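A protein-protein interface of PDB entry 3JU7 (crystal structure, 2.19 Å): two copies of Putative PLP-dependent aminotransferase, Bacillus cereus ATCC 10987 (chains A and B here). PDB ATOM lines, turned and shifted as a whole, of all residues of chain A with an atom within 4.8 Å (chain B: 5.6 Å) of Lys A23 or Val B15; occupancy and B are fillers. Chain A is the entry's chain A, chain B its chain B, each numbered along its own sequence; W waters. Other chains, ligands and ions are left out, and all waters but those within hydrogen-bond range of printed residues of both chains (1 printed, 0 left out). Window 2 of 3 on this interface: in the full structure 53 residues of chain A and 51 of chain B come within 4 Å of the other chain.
Water W1 lies within hydrogen-bond range of OD1 of Asp A26 (2.5 Å), OH of Tyr B18 (2.8 Å) and O of Val B13 (2.8 Å).
Val B15 touches just these residues of chain A: Leu A19, Leu A22, Lys A23 and Asp A26. Of the printed residues of chain A, Pro B14 touches Asp A26. Of the printed residues of chain B, Leu A22 touches Val B15. Printed residues of chain B within 4 Å of Leu A19: Val B15. Of the printed residues of chain B, Asp A26 touches Pro B14 (3.3 Å) and Val B15 (2.8 Å). The nearest printed residue of chain A that does not touch Val B15 is Glu A24 (7.5 Å). The nearest printed residue of chain B that does not touch Asp A26 is Val B13 (4.2 Å).
Among the printed residues, merely in contact across the chains: Leu A19 with Val B15, Leu A22 with Val B15, Lys A23 with Val B15 and Asp A26 with Pro B14.
Hydrophobic or aromatic side chains of chain B within 4 Å of the printed part of chain A: Pro B14 and Val B15. Printed residues of chain A that touch a printed residue of chain B: Leu A19, Leu A22, Lys A23 and Asp A26. Among the printed residues, 5 pairs touch across the chains. Among the printed residues, no Asp or Glu carboxylate lies within 4 Å of a Lys or Arg side-chain nitrogen of the other chain.
OD2 of Asp A26 lies within hydrogen-bond range of N of Val B15 (2.8 Å).
Positions printed for both chains: 19 and 22. Of the 5 pairs that touch across the chains among the printed residues, none has its exchanged pair printed and touching as well.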
ATOM      1  N   LEU A  19      20.740  -4.261 -21.012  1.00  0.00           N
ATOM      2  CA  LEU A  19      21.356  -4.861 -22.201  1.00  0.00           C
ATOM      3  C   LEU A  19      20.520  -6.050 -22.687  1.00  0.00           C
ATOM      4  O   LEU A  19      20.295  -6.192 -23.867  1.00  0.00           O
ATOM      5  CB  LEU A  19      22.808  -5.270 -21.925  1.00  0.00           C
ATOM      6  CG  LEU A  19      23.795  -5.470 -23.078  1.00  0.00           C
ATOM      7  CD1 LEU A  19      23.695  -4.343 -24.091  1.00  0.00           C
ATOM      8  CD2 LEU A  19      25.222  -5.518 -22.529  1.00  0.00           C
ATOM      9  N   ASP A  20      20.077  -6.902 -21.774  1.00  0.00           N
ATOM     10  CA  ASP A  20      19.104  -7.938 -22.111  1.00  0.00           C
ATOM     11  C   ASP A  20      17.922  -7.438 -22.923  1.00  0.00           C
ATOM     12  O   ASP A  20      17.548  -8.051 -23.896  1.00  0.00           O
ATOM     13  CB  ASP A  20      18.556  -8.567 -20.849  1.00  0.00           C
ATOM     14  CG  ASP A  20      19.565  -9.391 -20.147  1.00  0.00           C
ATOM     15  OD1 ASP A  20      20.661  -9.700 -20.702  1.00  0.00           O
ATOM     16  OD2 ASP A  20      19.264  -9.766 -19.021  1.00  0.00           O
ATOM     17  N   GLU A  21      17.336  -6.326 -22.527  1.00  0.00           N
ATOM     18  CA  GLU A  21      16.239  -5.781 -23.285  1.00  0.00           C
ATOM     19  C   GLU A  21      16.691  -5.329 -24.669  1.00  0.00           C
ATOM     20  O   GLU A  21      15.959  -5.535 -25.646  1.00  0.00           O
ATOM     21  CB  GLU A  21      15.560  -4.626 -22.546  1.00  0.00           C
ATOM     22  CG  GLU A  21      14.693  -5.071 -21.375  1.00  0.00           C
ATOM     23  CD  GLU A  21      15.488  -5.398 -20.115  1.00  0.00           C
ATOM     24  OE1 GLU A  21      16.700  -5.115 -20.057  1.00  0.00           O
ATOM     25  OE2 GLU A  21      14.897  -5.953 -19.177  1.00  0.00           O
ATOM     26  N   LEU A  22      17.871  -4.716 -24.759  1.00  0.00           N
ATOM     27  CA  LEU A  22      18.442  -4.361 -26.057  1.00  0.00           C
ATOM     28  C   LEU A  22      18.637  -5.612 -26.941  1.00  0.00           C
ATOM     29  O   LEU A  22      18.364  -5.573 -28.149  1.00  0.00           O
ATOM     30  CB  LEU A  22      19.763  -3.588 -25.902  1.00  0.00           C
ATOM     31  CG  LEU A  22      19.655  -2.209 -25.234  1.00  0.00           C
ATOM     32  CD1 LEU A  22      21.000  -1.512 -25.219  1.00  0.00           C
ATOM     33  CD2 LEU A  22      18.647  -1.321 -25.896  1.00  0.00           C
ATOM     34  N   LYS A  23      19.075  -6.728 -26.355  1.00  0.00           N
ATOM     35  CA  LYS A  23      19.130  -7.983 -27.121  1.00  0.00           C
ATOM     36  C   LYS A  23      17.739  -8.390 -27.590  1.00  0.00           C
ATOM     37  O   LYS A  23      17.563  -8.808 -28.723  1.00  0.00           O
ATOM     38  CB  LYS A  23      19.757  -9.146 -26.342  1.00  0.00           C
ATOM     39  CG  LYS A  23      21.234  -8.961 -25.958  1.00  0.00           C
ATOM     40  CD  LYS A  23      22.201  -8.548 -27.093  1.00  0.00           C
ATOM     41  CE  LYS A  23      22.690  -9.714 -27.966  1.00  0.00           C
ATOM     42  NZ  LYS A  23      24.048  -9.389 -28.542  1.00  0.00           N
ATOM     43  N   GLU A  24      16.736  -8.277 -26.731  1.00  0.00           N
ATOM     44  CA  GLU A  24      15.375  -8.581 -27.167  1.00  0.00           C
ATOM     45  C   GLU A  24      14.964  -7.746 -28.377  1.00  0.00           C
ATOM     46  O   GLU A  24      14.375  -8.264 -29.327  1.00  0.00           O
ATOM     47  CB  GLU A  24      14.394  -8.289 -26.070  1.00  0.00           C
ATOM     48  CG  GLU A  24      14.284  -9.342 -25.035  1.00  0.00           C
ATOM     49  CD  GLU A  24      13.116  -9.042 -24.129  1.00  0.00           C
ATOM     50  OE1 GLU A  24      11.961  -9.120 -24.605  1.00  0.00           O
ATOM     51  OE2 GLU A  24      13.365  -8.706 -22.961  1.00  0.00           O
ATOM     52  N   ILE A  25      15.244  -6.437 -28.317  1.00  0.00           N
ATOM     53  CA  ILE A  25      14.879  -5.561 -29.402  1.00  0.00           C
ATOM     54  C   ILE A  25      15.551  -5.997 -30.688  1.00  0.00           C
ATOM     55  O   ILE A  25      14.916  -6.033 -31.742  1.00  0.00           O
ATOM     56  CB  ILE A  25      15.286  -4.105 -29.127  1.00  0.00           C
ATOM     57  CG1 ILE A  25      14.397  -3.499 -28.027  1.00  0.00           C
ATOM     58  CG2 ILE A  25      15.154  -3.304 -30.383  1.00  0.00           C
ATOM     59  CD1 ILE A  25      14.966  -2.323 -27.283  1.00  0.00           C
ATOM     60  N   ASP A  26      16.835  -6.314 -30.616  1.00  0.00           N
ATOM     61  CA  ASP A  26      17.586  -6.717 -31.803  1.00  0.00           C
ATOM     62  C   ASP A  26      17.066  -8.047 -32.350  1.00  0.00           C
ATOM     63  O   ASP A  26      17.042  -8.222 -33.566  1.00  0.00           O
ATOM     64  CB  ASP A  26      19.090  -6.859 -31.514  1.00  0.00           C
ATOM     65  CG  ASP A  26      19.805  -5.519 -31.389  1.00  0.00           C
ATOM     66  OD1 ASP A  26      19.250  -4.516 -31.877  1.00  0.00           O
ATOM     67  OD2 ASP A  26      20.932  -5.493 -30.822  1.00  0.00           O
ATOM     68  N   ALA A  27      16.663  -8.970 -31.461  1.00  0.00           N
ATOM     69  CA  ALA A  27      16.095 -10.234 -31.915  1.00  0.00           C
ATOM     70  C   ALA A  27      14.700 -10.028 -32.520  1.00  0.00           C
ATOM     71  O   ALA A  27      14.358 -10.673 -33.476  1.00  0.00           O
ATOM     72  CB  ALA A  27      16.049 -11.265 -30.801  1.00  0.00           C
ATOM     73  N   VAL B  13      21.059  -1.129 -36.638  1.00  0.00           N
ATOM     74  CA  VAL B  13      22.345  -1.688 -36.214  1.00  0.00           C
ATOM     75  C   VAL B  13      22.207  -2.302 -34.820  1.00  0.00           C
ATOM     76  O   VAL B  13      21.530  -1.735 -33.968  1.00  0.00           O
ATOM     77  CB  VAL B  13      23.457  -0.631 -36.247  1.00  0.00           C
ATOM     78  CG1 VAL B  13      23.687  -0.156 -37.700  1.00  0.00           C
ATOM     79  CG2 VAL B  13      23.112   0.560 -35.394  1.00  0.00           C
ATOM     80  N   PRO B  14      22.797  -3.486 -34.601  1.00  0.00           N
ATOM     81  CA  PRO B  14      22.691  -4.149 -33.305  1.00  0.00           C
ATOM     82  C   PRO B  14      23.536  -3.493 -32.220  1.00  0.00           C
ATOM     83  O   PRO B  14      24.487  -2.763 -32.525  1.00  0.00           O
ATOM     84  CB  PRO B  14      23.223  -5.556 -33.580  1.00  0.00           C
ATOM     85  CG  PRO B  14      24.128  -5.398 -34.805  1.00  0.00           C
ATOM     86  CD  PRO B  14      23.443  -4.358 -35.614  1.00  0.00           C
ATOM     87  N   VAL B  15      23.205  -3.795 -30.965  1.00  0.00           N
ATOM     88  CA  VAL B  15      23.797  -3.094 -29.820  1.00  0.00           C
ATOM     89  C   VAL B  15      25.318  -3.076 -29.836  1.00  0.00           C
ATOM     90  O   VAL B  15      25.934  -2.068 -29.463  1.00  0.00           O
ATOM     91  CB  VAL B  15      23.244  -3.636 -28.458  1.00  0.00           C
ATOM     92  CG1 VAL B  15      23.423  -5.217 -28.307  1.00  0.00           C
ATOM     93  CG2 VAL B  15      23.850  -2.889 -27.326  1.00  0.00           C
ATOM     94  N   ILE B  16      25.948  -4.148 -30.303  1.00  0.00           N
ATOM     95  CA  ILE B  16      27.424  -4.154 -30.367  1.00  0.00           C
ATOM     96  C   ILE B  16      28.066  -2.961 -31.117  1.00  0.00           C
ATOM     97  O   ILE B  16      29.189  -2.581 -30.809  1.00  0.00           O
ATOM     98  CB  ILE B  16      27.987  -5.450 -30.956  1.00  0.00           C
ATOM     99  CG1 ILE B  16      29.416  -5.658 -30.461  1.00  0.00           C
ATOM    100  CG2 ILE B  16      27.904  -5.424 -32.496  1.00  0.00           C
ATOM    101  CD1 ILE B  16      29.568  -5.682 -28.925  1.00  0.00           C
ATOM    102  N   GLU B  17      27.346  -2.373 -32.069  1.00  0.00           N
ATOM    103  CA  GLU B  17      27.894  -1.324 -32.907  1.00  0.00           C
ATOM    104  C   GLU B  17      27.930   0.046 -32.225  1.00  0.00           C
ATOM    105  O   GLU B  17      28.713   0.906 -32.615  1.00  0.00           O
ATOM    106  CB  GLU B  17      27.100  -1.233 -34.200  1.00  0.00           C
ATOM    107  CG  GLU B  17      27.043  -2.529 -35.018  1.00  0.00           C
ATOM    108  CD  GLU B  17      28.400  -2.971 -35.521  1.00  0.00           C
ATOM    109  OE1 GLU B  17      29.329  -2.144 -35.526  1.00  0.00           O
ATOM    110  OE2 GLU B  17      28.546  -4.143 -35.908  1.00  0.00           O
ATOM    111  N   TYR B  18      27.060   0.258 -31.233  1.00  0.00           N
ATOM    112  CA  TYR B  18      27.024   1.518 -30.481  1.00  0.00           C
ATOM    113  C   TYR B  18      27.265   1.348 -28.962  1.00  0.00           C
ATOM    114  O   TYR B  18      27.127   2.312 -28.225  1.00  0.00           O
ATOM    115  CB  TYR B  18      25.710   2.263 -30.743  1.00  0.00           C
ATOM    116  CG  TYR B  18      24.446   1.469 -30.443  1.00  0.00           C
ATOM    117  CD1 TYR B  18      23.853   0.660 -31.409  1.00  0.00           C
ATOM    118  CD2 TYR B  18      23.830   1.556 -29.212  1.00  0.00           C
ATOM    119  CE1 TYR B  18      22.675  -0.049 -31.151  1.00  0.00           C
ATOM    120  CE2 TYR B  18      22.650   0.840 -28.934  1.00  0.00           C
ATOM    121  CZ  TYR B  18      22.087   0.038 -29.906  1.00  0.00           C
ATOM    122  OH  TYR B  18      20.947  -0.693 -29.623  1.00  0.00           O
ATOM    123  N   LEU B  19      27.640   0.152 -28.517  1.00  0.00           N
ATOM    124  CA  LEU B  19      28.010  -0.095 -27.111  1.00  0.00           C
ATOM    125  C   LEU B  19      29.124   0.819 -26.588  1.00  0.00           C
ATOM    126  O   LEU B  19      29.025   1.299 -25.466  1.00  0.00           O
ATOM    127  CB  LEU B  19      28.393  -1.579 -26.858  1.00  0.00           C
ATOM    128  CG  LEU B  19      28.505  -2.052 -25.397  1.00  0.00           C
ATOM    129  CD1 LEU B  19      27.241  -1.686 -24.552  1.00  0.00           C
ATOM    130  CD2 LEU B  19      28.861  -3.522 -25.262  1.00  0.00           C
ATOM    131  N   LEU B  22      27.455   4.029 -25.733  1.00  0.00           N
ATOM    132  CA  LEU B  22      26.636   3.906 -24.534  1.00  0.00           C
ATOM    133  C   LEU B  22      27.524   4.056 -23.303  1.00  0.00           C
ATOM    134  O   LEU B  22      27.219   4.832 -22.396  1.00  0.00           O
ATOM    135  CB  LEU B  22      25.863   2.592 -24.521  1.00  0.00           C
ATOM    136  CG  LEU B  22      24.838   2.439 -25.658  1.00  0.00           C
ATOM    137  CD1 LEU B  22      23.998   1.156 -25.499  1.00  0.00           C
ATOM    138  CD2 LEU B  22      23.921   3.697 -25.784  1.00  0.00           C
HETATM  139  O   HOH W   1      19.819  -2.072 -31.759  1.00  0.00           O
